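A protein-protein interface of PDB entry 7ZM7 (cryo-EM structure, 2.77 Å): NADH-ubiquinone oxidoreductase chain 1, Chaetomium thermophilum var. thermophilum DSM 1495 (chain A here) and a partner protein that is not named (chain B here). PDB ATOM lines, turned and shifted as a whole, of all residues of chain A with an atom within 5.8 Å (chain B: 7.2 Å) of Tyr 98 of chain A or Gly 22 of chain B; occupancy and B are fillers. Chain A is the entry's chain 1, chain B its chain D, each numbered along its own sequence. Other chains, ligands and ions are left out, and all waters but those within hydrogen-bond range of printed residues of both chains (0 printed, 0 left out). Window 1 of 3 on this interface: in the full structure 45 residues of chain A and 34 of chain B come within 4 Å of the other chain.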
ATOM      1  N   VAL A  16      -3.986 -20.111  -6.186  1.00  0.00           N
ATOM      2  CA  VAL A  16      -4.729 -21.354  -6.516  1.00  0.00           C
ATOM      3  C   VAL A  16      -4.937 -22.219  -5.265  1.00  0.00           C
ATOM      4  O   VAL A  16      -6.073 -22.640  -5.050  1.00  0.00           O
ATOM      5  CB  VAL A  16      -4.023 -22.121  -7.649  1.00  0.00           C
ATOM      6  CG1 VAL A  16      -4.638 -23.490  -7.891  1.00  0.00           C
ATOM      7  CG2 VAL A  16      -3.983 -21.322  -8.938  1.00  0.00           C
ATOM      8  N   SER A  20      -8.504 -23.090  -3.245  1.00  0.00           N
ATOM      9  CA  SER A  20      -8.827 -24.519  -3.457  1.00  0.00           C
ATOM     10  C   SER A  20      -9.003 -25.216  -2.110  1.00  0.00           C
ATOM     11  O   SER A  20      -9.975 -25.956  -1.968  1.00  0.00           O
ATOM     12  CB  SER A  20      -7.809 -25.216  -4.316  1.00  0.00           C
ATOM     13  OG  SER A  20      -7.870 -24.745  -5.652  1.00  0.00           O
ATOM     14  N   TYR A  93      -4.039 -29.940  -9.427  1.00  0.00           N
ATOM     15  CA  TYR A  93      -4.629 -28.587  -9.572  1.00  0.00           C
ATOM     16  C   TYR A  93      -3.681 -27.663 -10.325  1.00  0.00           C
ATOM     17  O   TYR A  93      -4.130 -26.601 -10.749  1.00  0.00           O
ATOM     18  CB  TYR A  93      -5.003 -28.016  -8.201  1.00  0.00           C
ATOM     19  CG  TYR A  93      -6.249 -28.581  -7.574  1.00  0.00           C
ATOM     20  CD1 TYR A  93      -6.236 -29.811  -6.935  1.00  0.00           C
ATOM     21  CD2 TYR A  93      -7.438 -27.874  -7.595  1.00  0.00           C
ATOM     22  CE1 TYR A  93      -7.377 -30.331  -6.349  1.00  0.00           C
ATOM     23  CE2 TYR A  93      -8.589 -28.380  -7.015  1.00  0.00           C
ATOM     24  CZ  TYR A  93      -8.558 -29.612  -6.390  1.00  0.00           C
ATOM     25  OH  TYR A  93      -9.684 -30.118  -5.815  1.00  0.00           O
ATOM     26  N   ILE A  96      -4.941 -26.816 -13.966  1.00  0.00           N
ATOM     27  CA  ILE A  96      -6.269 -26.254 -14.186  1.00  0.00           C
ATOM     28  C   ILE A  96      -6.192 -24.807 -14.656  1.00  0.00           C
ATOM     29  O   ILE A  96      -5.678 -23.943 -13.940  1.00  0.00           O
ATOM     30  CB  ILE A  96      -7.134 -26.374 -12.929  1.00  0.00           C
ATOM     31  CG1 ILE A  96      -6.918 -27.741 -12.265  1.00  0.00           C
ATOM     32  CG2 ILE A  96      -8.580 -26.077 -13.250  1.00  0.00           C
ATOM     33  CD1 ILE A  96      -7.213 -28.944 -13.151  1.00  0.00           C
ATOM     34  N   PRO A  97      -6.707 -24.505 -15.841  1.00  0.00           N
ATOM     35  CA  PRO A  97      -6.718 -23.122 -16.321  1.00  0.00           C
ATOM     36  C   PRO A  97      -7.955 -22.340 -15.907  1.00  0.00           C
ATOM     37  O   PRO A  97      -9.074 -22.778 -16.164  1.00  0.00           O
ATOM     38  CB  PRO A  97      -6.645 -23.298 -17.840  1.00  0.00           C
ATOM     39  CG  PRO A  97      -7.280 -24.623 -18.091  1.00  0.00           C
ATOM     40  CD  PRO A  97      -7.172 -25.455 -16.867  1.00  0.00           C
ATOM     41  N   TYR A  98      -7.780 -21.196 -15.261  1.00  0.00           N
ATOM     42  CA  TYR A  98      -8.893 -20.319 -14.895  1.00  0.00           C
ATOM     43  C   TYR A  98      -9.097 -19.203 -15.913  1.00  0.00           C
ATOM     44  O   TYR A  98      -9.277 -18.040 -15.568  1.00  0.00           O
ATOM     45  CB  TYR A  98      -8.665 -19.754 -13.504  1.00  0.00           C
ATOM     46  CG  TYR A  98      -8.480 -20.845 -12.481  1.00  0.00           C
ATOM     47  CD1 TYR A  98      -7.228 -21.381 -12.235  1.00  0.00           C
ATOM     48  CD2 TYR A  98      -9.554 -21.362 -11.791  1.00  0.00           C
ATOM     49  CE1 TYR A  98      -7.056 -22.368 -11.339  1.00  0.00           C
ATOM     50  CE2 TYR A  98      -9.387 -22.355 -10.887  1.00  0.00           C
ATOM     51  CZ  TYR A  98      -8.136 -22.855 -10.660  1.00  0.00           C
ATOM     52  OH  TYR A  98      -7.944 -23.859  -9.740  1.00  0.00           O
ATOM     53  N   GLY A  99      -9.041 -19.558 -17.196  1.00  0.00           N
ATOM     54  CA  GLY A  99      -9.116 -18.570 -18.286  1.00  0.00           C
ATOM     55  C   GLY A  99      -8.064 -18.990 -19.280  1.00  0.00           C
ATOM     56  O   GLY A  99      -7.296 -19.894 -18.923  1.00  0.00           O
ATOM     57  N   PRO A 100      -7.956 -18.416 -20.494  1.00  0.00           N
ATOM     58  CA  PRO A 100      -6.997 -18.949 -21.457  1.00  0.00           C
ATOM     59  C   PRO A 100      -5.556 -18.837 -20.952  1.00  0.00           C
ATOM     60  O   PRO A 100      -5.112 -17.754 -20.756  1.00  0.00           O
ATOM     61  CB  PRO A 100      -7.228 -18.060 -22.676  1.00  0.00           C
ATOM     62  CG  PRO A 100      -8.639 -17.547 -22.498  1.00  0.00           C
ATOM     63  CD  PRO A 100      -8.763 -17.321 -21.009  1.00  0.00           C
ATOM     64  N   LEU A 102      -4.437 -19.418 -18.151  1.00  0.00           N
ATOM     65  CA  LEU A 102      -4.329 -18.956 -16.771  1.00  0.00           C
ATOM     66  C   LEU A 102      -4.214 -20.134 -15.814  1.00  0.00           C
ATOM     67  O   LEU A 102      -5.080 -20.392 -14.986  1.00  0.00           O
ATOM     68  CB  LEU A 102      -5.521 -18.084 -16.416  1.00  0.00           C
ATOM     69  CG  LEU A 102      -5.490 -16.667 -16.963  1.00  0.00           C
ATOM     70  CD1 LEU A 102      -6.851 -16.054 -16.844  1.00  0.00           C
ATOM     71  CD2 LEU A 102      -4.461 -15.865 -16.215  1.00  0.00           C
ATOM     72  N   ALA A 103      -3.107 -20.850 -15.945  1.00  0.00           N
ATOM     73  CA  ALA A 103      -2.801 -21.996 -15.112  1.00  0.00           C
ATOM     74  C   ALA A 103      -1.430 -21.808 -14.497  1.00  0.00           C
ATOM     75  O   ALA A 103      -0.615 -21.021 -14.984  1.00  0.00           O
ATOM     76  CB  ALA A 103      -2.830 -23.298 -15.909  1.00  0.00           C
ATOM     77  N   ILE A 245     -13.822 -30.492 -11.693  1.00  0.00           N
ATOM     78  CA  ILE A 245     -13.270 -29.457 -12.557  1.00  0.00           C
ATOM     79  C   ILE A 245     -12.843 -30.054 -13.880  1.00  0.00           C
ATOM     80  O   ILE A 245     -13.058 -29.459 -14.938  1.00  0.00           O
ATOM     81  CB  ILE A 245     -12.094 -28.728 -11.890  1.00  0.00           C
ATOM     82  CG1 ILE A 245     -12.420 -28.339 -10.470  1.00  0.00           C
ATOM     83  CG2 ILE A 245     -11.777 -27.474 -12.648  1.00  0.00           C
ATOM     84  CD1 ILE A 245     -11.272 -27.770  -9.744  1.00  0.00           C
ATOM     85  N   TYR A 255     -14.165 -22.840 -18.802  1.00  0.00           N
ATOM     86  CA  TYR A 255     -14.402 -21.485 -18.335  1.00  0.00           C
ATOM     87  C   TYR A 255     -15.202 -20.672 -19.332  1.00  0.00           C
ATOM     88  O   TYR A 255     -15.262 -19.449 -19.223  1.00  0.00           O
ATOM     89  CB  TYR A 255     -13.075 -20.786 -18.034  1.00  0.00           C
ATOM     90  CG  TYR A 255     -12.022 -20.956 -19.104  1.00  0.00           C
ATOM     91  CD1 TYR A 255     -12.005 -20.150 -20.231  1.00  0.00           C
ATOM     92  CD2 TYR A 255     -11.041 -21.920 -18.981  1.00  0.00           C
ATOM     93  CE1 TYR A 255     -11.062 -20.316 -21.193  1.00  0.00           C
ATOM     94  CE2 TYR A 255     -10.086 -22.080 -19.930  1.00  0.00           C
ATOM     95  CZ  TYR A 255     -10.097 -21.284 -21.040  1.00  0.00           C
ATOM     96  OH  TYR A 255      -9.122 -21.467 -21.992  1.00  0.00           O
ATOM     97  N   PRO A 305      -8.697  -6.527 -16.974  1.00  0.00           N
ATOM     98  CA  PRO A 305      -8.131  -7.863 -16.778  1.00  0.00           C
ATOM     99  C   PRO A 305      -8.679  -8.574 -15.561  1.00  0.00           C
ATOM    100  O   PRO A 305      -8.651  -9.811 -15.526  1.00  0.00           O
ATOM    101  CB  PRO A 305      -6.629  -7.605 -16.623  1.00  0.00           C
ATOM    102  CG  PRO A 305      -6.443  -6.171 -16.572  1.00  0.00           C
ATOM    103  CD  PRO A 305      -7.713  -5.455 -16.788  1.00  0.00           C
ATOM    104  N   THR A 306      -9.150  -7.812 -14.576  1.00  0.00           N
ATOM    105  CA  THR A 306      -9.663  -8.425 -13.328  1.00  0.00           C
ATOM    106  C   THR A 306     -11.079  -8.937 -13.599  1.00  0.00           C
ATOM    107  O   THR A 306     -11.332 -10.106 -13.306  1.00  0.00           O
ATOM    108  CB  THR A 306      -9.573  -7.434 -12.165  1.00  0.00           C
ATOM    109  OG1 THR A 306      -8.234  -6.943 -12.119  1.00  0.00           O
ATOM    110  CG2 THR A 306      -9.937  -8.051 -10.833  1.00  0.00           C
ATOM    111  N   GLY A 309     -11.234 -11.982 -16.098  1.00  0.00           N
ATOM    112  CA  GLY A 309     -10.751 -13.161 -15.407  1.00  0.00           C
ATOM    113  C   GLY A 309     -11.740 -13.656 -14.377  1.00  0.00           C
ATOM    114  O   GLY A 309     -11.899 -14.861 -14.177  1.00  0.00           O
ATOM    115  N   SER A 310     -12.432 -12.727 -13.724  1.00  0.00           N
ATOM    116  CA  SER A 310     -13.408 -13.086 -12.710  1.00  0.00           C
ATOM    117  C   SER A 310     -14.534 -13.917 -13.305  1.00  0.00           C
ATOM    118  O   SER A 310     -14.985 -14.899 -12.706  1.00  0.00           O
ATOM    119  CB  SER A 310     -13.955 -11.818 -12.080  1.00  0.00           C
ATOM    120  OG  SER A 310     -12.893 -11.018 -11.624  1.00  0.00           O
ATOM    121  N   TYR A 312     -14.483 -15.680 -16.034  1.00  0.00           N
ATOM    122  CA  TYR A 312     -13.956 -16.967 -16.546  1.00  0.00           C
ATOM    123  C   TYR A 312     -13.897 -17.962 -15.383  1.00  0.00           C
ATOM    124  O   TYR A 312     -14.264 -19.132 -15.579  1.00  0.00           O
ATOM    125  CB  TYR A 312     -12.640 -16.757 -17.300  1.00  0.00           C
ATOM    126  CG  TYR A 312     -12.763 -16.363 -18.749  1.00  0.00           C
ATOM    127  CD1 TYR A 312     -13.950 -16.523 -19.440  1.00  0.00           C
ATOM    128  CD2 TYR A 312     -11.679 -15.852 -19.440  1.00  0.00           C
ATOM    129  CE1 TYR A 312     -14.063 -16.174 -20.776  1.00  0.00           C
ATOM    130  CE2 TYR A 312     -11.773 -15.494 -20.774  1.00  0.00           C
ATOM    131  CZ  TYR A 312     -12.971 -15.655 -21.447  1.00  0.00           C
ATOM    132  OH  TYR A 312     -13.072 -15.307 -22.762  1.00  0.00           O
ATOM    133  N   GLY A 313     -13.496 -17.504 -14.196  1.00  0.00           N
ATOM    134  CA  GLY A 313     -13.449 -18.379 -13.013  1.00  0.00           C
ATOM    135  C   GLY A 313     -14.799 -18.552 -12.350  1.00  0.00           C
ATOM    136  O   GLY A 313     -15.018 -19.644 -11.824  1.00  0.00           O
ATOM    137  N   LEU A 316     -16.281 -21.366 -14.493  1.00  0.00           N
ATOM    138  CA  LEU A 316     -15.741 -22.666 -14.136  1.00  0.00           C
ATOM    139  C   LEU A 316     -16.202 -23.084 -12.747  1.00  0.00           C
ATOM    140  O   LEU A 316     -16.446 -24.268 -12.498  1.00  0.00           O
ATOM    141  CB  LEU A 316     -14.223 -22.626 -14.224  1.00  0.00           C
ATOM    142  CG  LEU A 316     -13.517 -23.883 -13.748  1.00  0.00           C
ATOM    143  CD1 LEU A 316     -13.508 -24.932 -14.844  1.00  0.00           C
ATOM    144  CD2 LEU A 316     -12.125 -23.543 -13.283  1.00  0.00           C
ATOM    145  N   ALA B  16     -17.334 -18.268  -5.329  1.00  0.00           N
ATOM    146  CA  ALA B  16     -16.596 -17.023  -5.064  1.00  0.00           C
ATOM    147  C   ALA B  16     -15.090 -17.311  -5.047  1.00  0.00           C
ATOM    148  O   ALA B  16     -14.325 -16.453  -5.509  1.00  0.00           O
ATOM    149  CB  ALA B  16     -17.081 -16.421  -3.772  1.00  0.00           C
ATOM    150  N   MET B  17     -14.682 -18.490  -4.587  1.00  0.00           N
ATOM    151  CA  MET B  17     -13.243 -18.858  -4.516  1.00  0.00           C
ATOM    152  C   MET B  17     -12.694 -19.070  -5.923  1.00  0.00           C
ATOM    153  O   MET B  17     -11.574 -18.629  -6.185  1.00  0.00           O
ATOM    154  CB  MET B  17     -13.041 -20.099  -3.641  1.00  0.00           C
ATOM    155  CG  MET B  17     -13.341 -19.831  -2.186  1.00  0.00           C
ATOM    156  SD  MET B  17     -12.410 -18.397  -1.587  1.00  0.00           S
ATOM    157  CE  MET B  17     -13.741 -17.291  -1.124  1.00  0.00           C
ATOM    158  N   PHE B  18     -13.461 -19.745  -6.779  1.00  0.00           N
ATOM    159  CA  PHE B  18     -13.054 -19.949  -8.193  1.00  0.00           C
ATOM    160  C   PHE B  18     -12.982 -18.586  -8.880  1.00  0.00           C
ATOM    161  O   PHE B  18     -12.076 -18.376  -9.696  1.00  0.00           O
ATOM    162  CB  PHE B  18     -14.044 -20.880  -8.892  1.00  0.00           C
ATOM    163  CG  PHE B  18     -13.750 -22.351  -8.763  1.00  0.00           C
ATOM    164  CD1 PHE B  18     -14.126 -23.057  -7.635  1.00  0.00           C
ATOM    165  CD2 PHE B  18     -13.116 -23.036  -9.784  1.00  0.00           C
ATOM    166  CE1 PHE B  18     -13.862 -24.412  -7.522  1.00  0.00           C
ATOM    167  CE2 PHE B  18     -12.854 -24.391  -9.673  1.00  0.00           C
ATOM    168  CZ  PHE B  18     -13.227 -25.076  -8.542  1.00  0.00           C
ATOM    169  N   GLY B  19     -13.927 -17.702  -8.556  1.00  0.00           N
ATOM    170  CA  GLY B  19     -13.895 -16.340  -9.105  1.00  0.00           C
ATOM    171  C   GLY B  19     -12.643 -15.606  -8.685  1.00  0.00           C
ATOM    172  O   GLY B  19     -12.042 -14.975  -9.553  1.00  0.00           O
ATOM    173  N   VAL B  20     -12.243 -15.712  -7.413  1.00  0.00           N
ATOM    174  CA  VAL B  20     -11.061 -14.972  -6.876  1.00  0.00           C
ATOM    175  C   VAL B  20      -9.764 -15.517  -7.479  1.00  0.00           C
ATOM    176  O   VAL B  20      -8.864 -14.709  -7.734  1.00  0.00           O
ATOM    177  CB  VAL B  20     -11.032 -14.875  -5.333  1.00  0.00           C
ATOM    178  CG1 VAL B  20     -10.425 -16.095  -4.661  1.00  0.00           C
ATOM    179  CG2 VAL B  20     -10.323 -13.615  -4.865  1.00  0.00           C
ATOM    180  N   THR B  21      -9.665 -16.831  -7.677  1.00  0.00           N
ATOM    181  CA  THR B  21      -8.450 -17.391  -8.315  1.00  0.00           C
ATOM    182  C   THR B  21      -8.314 -16.842  -9.730  1.00  0.00           C
ATOM    183  O   THR B  21      -7.248 -16.335 -10.049  1.00  0.00           O
ATOM    184  CB  THR B  21      -8.493 -18.921  -8.383  1.00  0.00           C
ATOM    185  OG1 THR B  21      -8.611 -19.417  -7.050  1.00  0.00           O
ATOM    186  CG2 THR B  21      -7.272 -19.519  -9.047  1.00  0.00           C
ATOM    187  N   GLY B  22      -9.390 -16.856 -10.504  1.00  0.00           N
ATOM    188  CA  GLY B  22      -9.318 -16.407 -11.901  1.00  0.00           C
ATOM    189  C   GLY B  22      -9.192 -14.911 -11.945  1.00  0.00           C
ATOM    190  O   GLY B  22      -8.438 -14.412 -12.786  1.00  0.00           O
ATOM    191  N   ALA B  23      -9.920 -14.220 -11.073  1.00  0.00           N
ATOM    192  CA  ALA B  23      -9.786 -12.771 -10.983  1.00  0.00           C
ATOM    193  C   ALA B  23      -8.361 -12.370 -10.658  1.00  0.00           C
ATOM    194  O   ALA B  23      -7.758 -11.552 -11.355  1.00  0.00           O
ATOM    195  CB  ALA B  23     -10.719 -12.232  -9.913  1.00  0.00           C
ATOM    196  N   GLY B  24      -7.808 -12.945  -9.591  1.00  0.00           N
ATOM    197  CA  GLY B  24      -6.535 -12.475  -9.084  1.00  0.00           C
ATOM    198  C   GLY B  24      -5.365 -12.965  -9.898  1.00  0.00           C
ATOM    199  O   GLY B  24      -4.276 -12.404  -9.831  1.00  0.00           O
ATOM    200  N   MET B  25      -5.559 -14.049 -10.644  1.00  0.00           N
ATOM    201  CA  MET B  25      -4.448 -14.638 -11.442  1.00  0.00           C
ATOM    202  C   MET B  25      -4.343 -13.911 -12.783  1.00  0.00           C
ATOM    203  O   MET B  25      -3.231 -13.806 -13.306  1.00  0.00           O
ATOM    204  CB  MET B  25      -4.689 -16.127 -11.675  1.00  0.00           C
ATOM    205  CG  MET B  25      -3.414 -16.919 -11.864  1.00  0.00           C
ATOM    206  SD  MET B  25      -3.584 -18.611 -11.262  1.00  0.00           S
ATOM    207  CE  MET B  25      -2.256 -19.411 -12.155  1.00  0.00           C
ATOM    208  N   ALA B  26      -5.470 -13.452 -13.324  1.00  0.00           N
ATOM    209  CA  ALA B  26      -5.467 -12.679 -14.584  1.00  0.00           C
ATOM    210  C   ALA B  26      -4.762 -11.345 -14.363  1.00  0.00           C
ATOM    211  O   ALA B  26      -4.141 -10.851 -15.315  1.00  0.00           O
ATOM    212  CB  ALA B  26      -6.869 -12.504 -15.110  1.00  0.00           C
ATOM    213  N   LYS B  27      -4.869 -10.780 -13.163  1.00  0.00           N
ATOM    214  CA  LYS B  27      -4.299  -9.433 -12.934  1.00  0.00           C
ATOM    215  C   LYS B  27      -2.802  -9.541 -12.642  1.00  0.00           C
ATOM    216  O   LYS B  27      -2.059  -8.735 -13.206  1.00  0.00           O
ATOM    217  CB  LYS B  27      -5.053  -8.731 -11.802  1.00  0.00           C
ATOM    218  CG  LYS B  27      -4.579  -7.324 -11.467  1.00  0.00           C
ATOM    219  CD  LYS B  27      -4.528  -6.402 -12.664  1.00  0.00           C
ATOM    220  CE  LYS B  27      -3.905  -5.060 -12.347  1.00  0.00           C
ATOM    221  NZ  LYS B  27      -3.634  -4.276 -13.575  1.00  0.00           N
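The backbone carbonyl oxygen (O) of Val 16 of chain A lies within hydrogen-bond range of the side-chain hydroxyl (OG) of Ser 20 of chain A (2.8 Å). The backbone carbonyl oxygen (O) of Met 17 of chain B sits at hydrogen-bond distance from the side-chain hydroxyl (OG1) of Thr 21 of chain B (3.2 Å). The backbone carbonyl oxygen (O) of Thr 306 of chain A lies within hydrogen-bond range of the side-chain hydroxyl (OG) of Ser 310 of chain A (2.5 Å).
Of chain B, only Phe 18 (3.9 Å), Thr 21 (3.7 Å) and Gly 22 (3.8 Å) come within 4 Å of Tyr 98 of chain A. Of the printed residues of chain A, Gly 22 of chain B touches Tyr 98 (3.8 Å) and Gly 309 (3.5 Å). Printed residues of chain B within 4 Å of Leu 102 of chain A: Met 25 and Ala 26. Of the printed residues of chain A, Ala 23 of chain B touches Thr 306, Gly 309 and Ser 310. Of the printed residues of chain B, Ile 245 of chain A touches Phe 18. Printed residues of chain B within 4 Å of Ser 310 of chain A: Gly 19 and Ala 23. The nearest residue of chain B that does not touch Tyr 98 of chain A is Met 25 of chain B (4.7 Å). The nearest printed residue of chain A that does not touch Phe 18 of chain B is Ser 310 of chain A (5.4 Å).
CG2 of Val 16 of chain A touches SD of Met 25 of chain B, 3.6 Å away. CD2 of Phe 18 of chain B touches CE2 of Tyr 98 of chain A, 3.9 Å away. Ala 103 of chain A touches Met 25 of chain B (C to CE, 3.5 Å). Phe 18 of chain B touches Ile 245 of chain A. Pro 305 of chain A touches Ala 26 of chain B (O to CB, 3.3 Å). CB of Lys 27 of chain B touches OG1 of Thr 306 of chain A, 3.7 Å away. Ala 26 of chain B touches Gly 309 of chain A (CB to CA, 3.9 Å). Gly 19 of chain B touches Ser 310 of chain A (O to CA, 3.9 Å). Gly 313 of chain A touches Phe 18 of chain B (O to CB, 3.3 Å). Leu 316 of chain A touches Phe 18 of chain B.
Printed residues of chain A that touch a printed residue of chain B: Val 16, Tyr 98, Leu 102, Ala 103, Ile 245, Pro 305, Thr 306, Gly 309, Ser 310, Gly 313 and Leu 316. Hydrophobic or aromatic side chains of chain A that line the printed part of chain B: Val 16, Tyr 98, Leu 102, Ile 245 and Leu 316. Of the 12 printed residues of chain B, 8 touch a printed residue of chain A. Printed residues of chain B that touch a printed residue of chain A: Phe 18, Gly 19, Thr 21, Gly 22, Ala 23, Met 25, Ala 26 and Lys 27. Hydrophobic or aromatic side chains of chain B that line the printed part of chain A: Phe 18, Ala 23, Met 25 and Ala 26. Among the printed residues, 20 pairs touch across the chains. Among the printed residues, no Asp or Glu carboxylate lies within 4 Å of a Lys or Arg side-chain nitrogen of the other chain.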
